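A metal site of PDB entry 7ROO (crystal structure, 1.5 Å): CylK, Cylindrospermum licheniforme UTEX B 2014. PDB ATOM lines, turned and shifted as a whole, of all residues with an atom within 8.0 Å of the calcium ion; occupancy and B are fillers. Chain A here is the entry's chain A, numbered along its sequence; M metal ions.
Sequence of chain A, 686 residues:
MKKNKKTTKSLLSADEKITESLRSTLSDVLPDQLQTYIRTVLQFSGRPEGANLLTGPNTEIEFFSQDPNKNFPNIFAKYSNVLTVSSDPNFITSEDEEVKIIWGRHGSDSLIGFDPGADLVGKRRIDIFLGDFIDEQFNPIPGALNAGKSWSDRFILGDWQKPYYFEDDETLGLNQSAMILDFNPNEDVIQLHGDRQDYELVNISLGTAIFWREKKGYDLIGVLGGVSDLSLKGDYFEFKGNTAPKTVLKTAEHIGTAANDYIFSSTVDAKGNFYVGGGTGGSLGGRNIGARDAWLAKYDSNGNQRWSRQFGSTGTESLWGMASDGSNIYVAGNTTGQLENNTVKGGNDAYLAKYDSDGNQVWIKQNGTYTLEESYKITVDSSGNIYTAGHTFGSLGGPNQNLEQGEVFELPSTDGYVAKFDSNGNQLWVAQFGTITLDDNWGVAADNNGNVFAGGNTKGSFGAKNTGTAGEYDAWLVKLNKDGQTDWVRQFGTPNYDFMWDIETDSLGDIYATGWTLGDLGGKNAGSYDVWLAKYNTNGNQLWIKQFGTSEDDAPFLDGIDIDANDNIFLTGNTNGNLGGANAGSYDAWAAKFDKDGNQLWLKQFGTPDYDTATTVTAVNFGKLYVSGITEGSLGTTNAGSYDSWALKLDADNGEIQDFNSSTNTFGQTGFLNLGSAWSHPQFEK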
ATOM      1  N   PHE A 114     -15.955 -32.950   5.442  1.00  0.00           N
ATOM      2  CA  PHE A 114     -15.655 -31.528   5.164  1.00  0.00           C
ATOM      3  C   PHE A 114     -15.773 -30.739   6.453  1.00  0.00           C
ATOM      4  O   PHE A 114     -16.749 -30.919   7.228  1.00  0.00           O
ATOM      5  CB  PHE A 114     -16.598 -31.068   4.072  1.00  0.00           C
ATOM      6  CG  PHE A 114     -16.323 -29.739   3.443  1.00  0.00           C
ATOM      7  CD1 PHE A 114     -15.396 -29.646   2.422  1.00  0.00           C
ATOM      8  CD2 PHE A 114     -16.938 -28.591   3.903  1.00  0.00           C
ATOM      9  CE1 PHE A 114     -15.154 -28.438   1.784  1.00  0.00           C
ATOM     10  CE2 PHE A 114     -16.697 -27.395   3.246  1.00  0.00           C
ATOM     11  CZ  PHE A 114     -15.785 -27.336   2.221  1.00  0.00           C
ATOM     12  N   ARG A 125     -10.286 -30.733  -2.823  1.00  0.00           N
ATOM     13  CA  ARG A 125     -10.836 -31.565  -1.739  1.00  0.00           C
ATOM     14  C   ARG A 125     -11.761 -32.608  -2.356  1.00  0.00           C
ATOM     15  O   ARG A 125     -12.880 -32.258  -2.804  1.00  0.00           O
ATOM     16  CB  ARG A 125     -11.570 -30.699  -0.713  1.00  0.00           C
ATOM     17  CG  ARG A 125     -10.624 -29.976   0.229  1.00  0.00           C
ATOM     18  CD  ARG A 125      -9.816 -30.873   1.114  1.00  0.00           C
ATOM     19  NE  ARG A 125     -10.897 -31.276   2.007  1.00  0.00           N
ATOM     20  CZ  ARG A 125     -11.495 -32.478   2.097  1.00  0.00           C
ATOM     21  NH1 ARG A 125     -11.092 -33.550   1.384  1.00  0.00           N
ATOM     22  NH2 ARG A 125     -12.560 -32.539   2.890  1.00  0.00           N
ATOM     23  N   TYR A 164     -21.540 -27.987   1.482  1.00  0.00           N
ATOM     24  CA  TYR A 164     -20.123 -28.360   1.551  1.00  0.00           C
ATOM     25  C   TYR A 164     -19.532 -28.495   0.152  1.00  0.00           C
ATOM     26  O   TYR A 164     -20.273 -28.643  -0.868  1.00  0.00           O
ATOM     27  CB  TYR A 164     -19.992 -29.642   2.367  1.00  0.00           C
ATOM     28  CG  TYR A 164     -20.385 -29.535   3.810  1.00  0.00           C
ATOM     29  CD1 TYR A 164     -20.729 -28.331   4.405  1.00  0.00           C
ATOM     30  CD2 TYR A 164     -20.410 -30.667   4.589  1.00  0.00           C
ATOM     31  CE1 TYR A 164     -21.115 -28.256   5.739  1.00  0.00           C
ATOM     32  CE2 TYR A 164     -20.782 -30.608   5.934  1.00  0.00           C
ATOM     33  CZ  TYR A 164     -21.117 -29.414   6.508  1.00  0.00           C
ATOM     34  OH  TYR A 164     -21.470 -29.364   7.830  1.00  0.00           O
ATOM     35  N   TYR A 165     -18.217 -28.416   0.033  1.00  0.00           N
ATOM     36  CA  TYR A 165     -17.531 -28.646  -1.275  1.00  0.00           C
ATOM     37  C   TYR A 165     -17.928 -27.547  -2.261  1.00  0.00           C
ATOM     38  O   TYR A 165     -17.937 -27.795  -3.440  1.00  0.00           O
ATOM     39  CB  TYR A 165     -17.768 -30.043  -1.847  1.00  0.00           C
ATOM     40  CG  TYR A 165     -17.570 -31.169  -0.848  1.00  0.00           C
ATOM     41  CD1 TYR A 165     -16.309 -31.662  -0.555  1.00  0.00           C
ATOM     42  CD2 TYR A 165     -18.635 -31.739  -0.211  1.00  0.00           C
ATOM     43  CE1 TYR A 165     -16.109 -32.693   0.369  1.00  0.00           C
ATOM     44  CE2 TYR A 165     -18.489 -32.737   0.738  1.00  0.00           C
ATOM     45  CZ  TYR A 165     -17.213 -33.207   1.025  1.00  0.00           C
ATOM     46  OH  TYR A 165     -17.029 -34.200   1.957  1.00  0.00           O
ATOM     47  N   PHE A 166     -18.200 -26.358  -1.747  1.00  0.00           N
ATOM     48  CA  PHE A 166     -18.767 -25.243  -2.565  1.00  0.00           C
ATOM     49  C   PHE A 166     -17.712 -24.168  -2.759  1.00  0.00           C
ATOM     50  O   PHE A 166     -17.253 -23.555  -1.768  1.00  0.00           O
ATOM     51  CB  PHE A 166     -20.032 -24.740  -1.879  1.00  0.00           C
ATOM     52  CG  PHE A 166     -20.699 -23.615  -2.613  1.00  0.00           C
ATOM     53  CD1 PHE A 166     -21.213 -23.827  -3.873  1.00  0.00           C
ATOM     54  CD2 PHE A 166     -20.901 -22.410  -1.979  1.00  0.00           C
ATOM     55  CE1 PHE A 166     -21.842 -22.790  -4.539  1.00  0.00           C
ATOM     56  CE2 PHE A 166     -21.567 -21.390  -2.637  1.00  0.00           C
ATOM     57  CZ  PHE A 166     -22.031 -21.603  -3.905  1.00  0.00           C
ATOM     58  N   GLU A 167     -17.354 -23.955  -4.026  1.00  0.00           N
ATOM     59  CA  GLU A 167     -16.316 -22.998  -4.435  1.00  0.00           C
ATOM     60  C   GLU A 167     -16.933 -21.645  -4.840  1.00  0.00           C
ATOM     61  O   GLU A 167     -16.155 -20.695  -4.739  1.00  0.00           O
ATOM     62  CB  GLU A 167     -15.440 -23.591  -5.550  1.00  0.00           C
ATOM     63  CG  GLU A 167     -14.669 -24.839  -5.112  1.00  0.00           C
ATOM     64  CD  GLU A 167     -14.861 -25.990  -6.060  1.00  0.00           C
ATOM     65  OE1 GLU A 167     -14.269 -25.900  -7.173  1.00  0.00           O
ATOM     66  OE2 GLU A 167     -15.682 -26.924  -5.738  1.00  0.00           O
ATOM     67  N   ASP A 168     -18.220 -21.582  -5.182  1.00  0.00           N
ATOM     68  CA  ASP A 168     -18.952 -20.288  -5.357  1.00  0.00           C
ATOM     69  C   ASP A 168     -18.168 -19.411  -6.350  1.00  0.00           C
ATOM     70  O   ASP A 168     -17.704 -18.318  -5.966  1.00  0.00           O
ATOM     71  CB  ASP A 168     -19.102 -19.563  -4.024  1.00  0.00           C
ATOM     72  CG  ASP A 168     -20.096 -18.402  -4.008  1.00  0.00           C
ATOM     73  OD1 ASP A 168     -20.863 -18.233  -4.976  1.00  0.00           O
ATOM     74  OD2 ASP A 168     -20.113 -17.694  -2.989  1.00  0.00           O
ATOM     75  N   ASP A 169     -17.977 -19.901  -7.568  1.00  0.00           N
ATOM     76  CA  ASP A 169     -17.120 -19.228  -8.586  1.00  0.00           C
ATOM     77  C   ASP A 169     -17.635 -19.527  -9.998  1.00  0.00           C
ATOM     78  O   ASP A 169     -18.696 -20.086 -10.138  1.00  0.00           O
ATOM     79  CB  ASP A 169     -15.646 -19.590  -8.415  1.00  0.00           C
ATOM     80  CG  ASP A 169     -15.251 -21.014  -8.763  1.00  0.00           C
ATOM     81  OD1 ASP A 169     -16.038 -21.702  -9.469  1.00  0.00           O
ATOM     82  OD2 ASP A 169     -14.120 -21.402  -8.403  1.00  0.00           O
ATOM     83  N   THR A 171     -16.450 -21.380 -12.368  1.00  0.00           N
ATOM     84  CA  THR A 171     -16.227 -22.779 -12.846  1.00  0.00           C
ATOM     85  C   THR A 171     -17.408 -23.666 -12.475  1.00  0.00           C
ATOM     86  O   THR A 171     -18.306 -23.193 -11.780  1.00  0.00           O
ATOM     87  CB  THR A 171     -14.917 -23.348 -12.295  1.00  0.00           C
ATOM     88  OG1 THR A 171     -15.118 -23.715 -10.930  1.00  0.00           O
ATOM     89  CG2 THR A 171     -13.763 -22.371 -12.430  1.00  0.00           C
ATOM     90  N   LEU A 172     -17.401 -24.932 -12.938  1.00  0.00           N
ATOM     91  CA  LEU A 172     -18.413 -25.952 -12.504  1.00  0.00           C
ATOM     92  C   LEU A 172     -18.113 -26.376 -11.044  1.00  0.00           C
ATOM     93  O   LEU A 172     -18.884 -27.157 -10.525  1.00  0.00           O
ATOM     94  CB  LEU A 172     -18.427 -27.159 -13.431  1.00  0.00           C
ATOM     95  CG  LEU A 172     -19.113 -26.963 -14.792  1.00  0.00           C
ATOM     96  CD1 LEU A 172     -18.964 -28.202 -15.648  1.00  0.00           C
ATOM     97  CD2 LEU A 172     -20.569 -26.593 -14.620  1.00  0.00           C
ATOM     98  N   GLY A 173     -17.049 -25.878 -10.416  1.00  0.00           N
ATOM     99  CA  GLY A 173     -16.848 -26.158  -8.970  1.00  0.00           C
ATOM    100  C   GLY A 173     -16.405 -27.592  -8.814  1.00  0.00           C
ATOM    101  O   GLY A 173     -16.983 -28.310  -7.955  1.00  0.00           O
ATOM    102  N   LEU A 174     -15.420 -28.006  -9.602  1.00  0.00           N
ATOM    103  CA  LEU A 174     -14.951 -29.413  -9.627  1.00  0.00           C
ATOM    104  C   LEU A 174     -13.753 -29.616  -8.700  1.00  0.00           C
ATOM    105  O   LEU A 174     -13.290 -30.749  -8.547  1.00  0.00           O
ATOM    106  CB  LEU A 174     -14.606 -29.774 -11.070  1.00  0.00           C
ATOM    107  CG  LEU A 174     -15.678 -29.456 -12.102  1.00  0.00           C
ATOM    108  CD1 LEU A 174     -15.253 -29.907 -13.474  1.00  0.00           C
ATOM    109  CD2 LEU A 174     -17.040 -30.043 -11.765  1.00  0.00           C
ATOM    110  N   ASN A 175     -13.206 -28.530  -8.144  1.00  0.00           N
ATOM    111  CA  ASN A 175     -12.004 -28.620  -7.315  1.00  0.00           C
ATOM    112  C   ASN A 175     -12.339 -29.302  -5.978  1.00  0.00           C
ATOM    113  O   ASN A 175     -11.459 -29.955  -5.433  1.00  0.00           O
ATOM    114  CB  ASN A 175     -11.429 -27.222  -7.162  1.00  0.00           C
ATOM    115  CG  ASN A 175      -9.939 -27.223  -7.185  1.00  0.00           C
ATOM    116  OD1 ASN A 175      -9.332 -27.918  -8.001  1.00  0.00           O
ATOM    117  ND2 ASN A 175      -9.341 -26.439  -6.290  1.00  0.00           N
ATOM    118  N   GLN A 176     -13.607 -29.204  -5.533  1.00  0.00           N
ATOM    119  CA  GLN A 176     -14.074 -29.784  -4.251  1.00  0.00           C
ATOM    120  C   GLN A 176     -15.360 -30.556  -4.543  1.00  0.00           C
ATOM    121  O   GLN A 176     -16.306 -29.986  -5.078  1.00  0.00           O
ATOM    122  CB  GLN A 176     -14.286 -28.718  -3.168  1.00  0.00           C
ATOM    123  CG  GLN A 176     -13.045 -27.870  -2.941  1.00  0.00           C
ATOM    124  CD  GLN A 176     -13.212 -26.892  -1.802  1.00  0.00           C
ATOM    125  OE1 GLN A 176     -14.307 -26.700  -1.273  1.00  0.00           O
ATOM    126  NE2 GLN A 176     -12.105 -26.272  -1.452  1.00  0.00           N
ATOM    127  N   SER A 177     -15.416 -31.801  -4.112  1.00  0.00           N
ATOM    128  CA  SER A 177     -16.616 -32.645  -4.274  1.00  0.00           C
ATOM    129  C   SER A 177     -16.551 -33.845  -3.347  1.00  0.00           C
ATOM    130  O   SER A 177     -15.476 -34.305  -3.082  1.00  0.00           O
ATOM    131  CB  SER A 177     -16.685 -33.095  -5.703  1.00  0.00           C
ATOM    132  OG  SER A 177     -17.890 -33.792  -5.926  1.00  0.00           O
ATOM    133  N   ALA A 178     -17.690 -34.329  -2.925  1.00  0.00           N
ATOM    134  CA  ALA A 178     -17.806 -35.696  -2.366  1.00  0.00           C
ATOM    135  C   ALA A 178     -17.899 -36.714  -3.500  1.00  0.00           C
ATOM    136  O   ALA A 178     -18.413 -36.428  -4.614  1.00  0.00           O
ATOM    137  CB  ALA A 178     -19.016 -35.810  -1.513  1.00  0.00           C
ATOM    138  N   ILE A 210     -24.580 -34.355  -8.198  1.00  0.00           N
ATOM    139  CA  ILE A 210     -25.405 -33.372  -7.460  1.00  0.00           C
ATOM    140  C   ILE A 210     -24.770 -31.997  -7.630  1.00  0.00           C
ATOM    141  O   ILE A 210     -23.659 -31.730  -7.141  1.00  0.00           O
ATOM    142  CB  ILE A 210     -25.506 -33.745  -5.945  1.00  0.00           C
ATOM    143  CG1 ILE A 210     -25.982 -35.182  -5.689  1.00  0.00           C
ATOM    144  CG2 ILE A 210     -26.369 -32.756  -5.181  1.00  0.00           C
ATOM    145  CD1 ILE A 210     -25.842 -35.614  -4.214  1.00  0.00           C
ATOM    146  N   PHE A 211     -25.443 -31.084  -8.323  1.00  0.00           N
ATOM    147  CA  PHE A 211     -24.993 -29.703  -8.486  1.00  0.00           C
ATOM    148  C   PHE A 211     -25.824 -28.763  -7.649  1.00  0.00           C
ATOM    149  O   PHE A 211     -27.061 -28.880  -7.649  1.00  0.00           O
ATOM    150  CB  PHE A 211     -25.140 -29.283  -9.959  1.00  0.00           C
ATOM    151  CG  PHE A 211     -23.997 -29.697 -10.843  1.00  0.00           C
ATOM    152  CD1 PHE A 211     -22.795 -29.011 -10.822  1.00  0.00           C
ATOM    153  CD2 PHE A 211     -24.109 -30.806 -11.646  1.00  0.00           C
ATOM    154  CE1 PHE A 211     -21.764 -29.380 -11.654  1.00  0.00           C
ATOM    155  CE2 PHE A 211     -23.056 -31.209 -12.446  1.00  0.00           C
ATOM    156  CZ  PHE A 211     -21.882 -30.500 -12.445  1.00  0.00           C
ATOM    157  N   TRP A 212     -25.155 -27.873  -6.942  1.00  0.00           N
ATOM    158  CA  TRP A 212     -25.752 -26.643  -6.415  1.00  0.00           C
ATOM    159  C   TRP A 212     -26.029 -25.749  -7.626  1.00  0.00           C
ATOM    160  O   TRP A 212     -25.141 -25.608  -8.413  1.00  0.00           O
ATOM    161  CB  TRP A 212     -24.828 -25.958  -5.403  1.00  0.00           C
ATOM    162  CG  TRP A 212     -25.357 -24.670  -4.842  1.00  0.00           C
ATOM    163  CD1 TRP A 212     -25.063 -23.448  -5.348  1.00  0.00           C
ATOM    164  CD2 TRP A 212     -26.241 -24.459  -3.736  1.00  0.00           C
ATOM    165  NE1 TRP A 212     -25.703 -22.482  -4.625  1.00  0.00           N
ATOM    166  CE2 TRP A 212     -26.436 -23.062  -3.629  1.00  0.00           C
ATOM    167  CE3 TRP A 212     -26.900 -25.276  -2.791  1.00  0.00           C
ATOM    168  CZ2 TRP A 212     -27.224 -22.495  -2.626  1.00  0.00           C
ATOM    169  CZ3 TRP A 212     -27.694 -24.714  -1.827  1.00  0.00           C
ATOM    170  CH2 TRP A 212     -27.896 -23.335  -1.778  1.00  0.00           C
ATOM    171  N   TYR A 218     -23.448 -22.959 -11.374  1.00  0.00           N
ATOM    172  CA  TYR A 218     -23.469 -24.368 -10.906  1.00  0.00           C
ATOM    173  C   TYR A 218     -22.207 -24.654 -10.111  1.00  0.00           C
ATOM    174  O   TYR A 218     -21.139 -24.145 -10.444  1.00  0.00           O
ATOM    175  CB  TYR A 218     -23.508 -25.340 -12.096  1.00  0.00           C
ATOM    176  CG  TYR A 218     -24.833 -25.426 -12.801  1.00  0.00           C
ATOM    177  CD1 TYR A 218     -25.147 -24.585 -13.866  1.00  0.00           C
ATOM    178  CD2 TYR A 218     -25.776 -26.334 -12.392  1.00  0.00           C
ATOM    179  CE1 TYR A 218     -26.377 -24.675 -14.503  1.00  0.00           C
ATOM    180  CE2 TYR A 218     -27.013 -26.423 -13.008  1.00  0.00           C
ATOM    181  CZ  TYR A 218     -27.314 -25.600 -14.073  1.00  0.00           C
ATOM    182  OH  TYR A 218     -28.539 -25.764 -14.640  1.00  0.00           O
ATOM    183  N   ASP A 219     -22.307 -25.575  -9.135  1.00  0.00           N
ATOM    184  CA  ASP A 219     -21.124 -26.034  -8.376  1.00  0.00           C
ATOM    185  C   ASP A 219     -21.311 -27.509  -8.036  1.00  0.00           C
ATOM    186  O   ASP A 219     -22.356 -27.838  -7.394  1.00  0.00           O
ATOM    187  CB  ASP A 219     -20.910 -25.213  -7.100  1.00  0.00           C
ATOM    188  CG  ASP A 219     -19.533 -25.416  -6.507  1.00  0.00           C
ATOM    189  OD1 ASP A 219     -19.241 -26.586  -6.190  1.00  0.00           O
ATOM    190  OD2 ASP A 219     -18.730 -24.481  -6.398  1.00  0.00           O
ATOM    191  N   LEU A 220     -20.368 -28.351  -8.434  1.00  0.00           N
ATOM    192  CA  LEU A 220     -20.490 -29.795  -8.109  1.00  0.00           C
ATOM    193  C   LEU A 220     -20.326 -30.022  -6.583  1.00  0.00           C
ATOM    194  O   LEU A 220     -19.310 -29.625  -6.036  1.00  0.00           O
ATOM    195  CB  LEU A 220     -19.457 -30.587  -8.884  1.00  0.00           C
ATOM    196  CG  LEU A 220     -19.474 -32.086  -8.598  1.00  0.00           C
ATOM    197  CD1 LEU A 220     -20.758 -32.737  -9.111  1.00  0.00           C
ATOM    198  CD2 LEU A 220     -18.228 -32.714  -9.173  1.00  0.00           C
ATOM    199  N   ILE A 221     -21.325 -30.597  -5.924  1.00  0.00           N
ATOM    200  CA  ILE A 221     -21.277 -30.875  -4.466  1.00  0.00           C
ATOM    201  C   ILE A 221     -20.865 -32.332  -4.281  1.00  0.00           C
ATOM    202  O   ILE A 221     -20.015 -32.609  -3.414  1.00  0.00           O
ATOM    203  CB  ILE A 221     -22.602 -30.558  -3.776  1.00  0.00           C
ATOM    204  CG1 ILE A 221     -23.054 -29.115  -4.024  1.00  0.00           C
ATOM    205  CG2 ILE A 221     -22.542 -30.870  -2.284  1.00  0.00           C
ATOM    206  CD1 ILE A 221     -22.006 -28.076  -3.772  1.00  0.00           C
ATOM    207  N   GLY A 222     -21.400 -33.257  -5.075  1.00  0.00           N
ATOM    208  CA  GLY A 222     -21.071 -34.682  -4.923  1.00  0.00           C
ATOM    209  C   GLY A 222     -21.403 -35.517  -6.118  1.00  0.00           C
ATOM    210  O   GLY A 222     -22.279 -35.147  -6.922  1.00  0.00           O
HETATM  211 CA    CA M   1     -17.593 -28.151  -5.700  1.00  0.00          CA
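The backbone NH of Leu 174 is in hydrogen-bond range of the side-chain carboxylate of Glu 167 (3.4 Å). The side-chain carboxylate (OE1) of Glu 167 lies within hydrogen-bond range of the backbone NH (N) of Asn 175 (3.0 Å). The backbone carbonyl oxygen (O) of Leu 172 sits at hydrogen-bond distance from the backbone NH (N) of Leu 220 (2.8 Å). The side-chain carboxylate (OD2) of Asp 219 sits at hydrogen-bond distance from the backbone NH (N) of Asp 168 (3.2 Å). N of Trp 212 sits at hydrogen-bond distance from O of Asp 219 (2.8 Å). N of Gly 173 lies within hydrogen-bond range of OG1 of Thr 171 (2.9 Å).
Of the 24 residues printed, 6 come within 4 Å of the calcium ion. Along chain A the residues within 4 Å of the calcium ion span positions 165 to 220. The nearest printed residue that does not touch the calcium ion is Phe 166 (4.4 Å).
The calcium ion is bound by OE2 of Glu 167 (2.3 Å). The calcium ion is bound by O of Leu 220 (2.3 Å). The calcium ion is bound by O of Tyr 165, 2.3 Å away. The side-chain carboxylate (OD1) of Asp 219 binds the calcium ion (2.3 Å). The calcium ion is bound by the backbone carbonyl oxygen (O) of Gln 176, 2.3 Å away. The calcium ion is bound by the backbone carbonyl oxygen (O) of Gly 173, at 2.3 Å.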
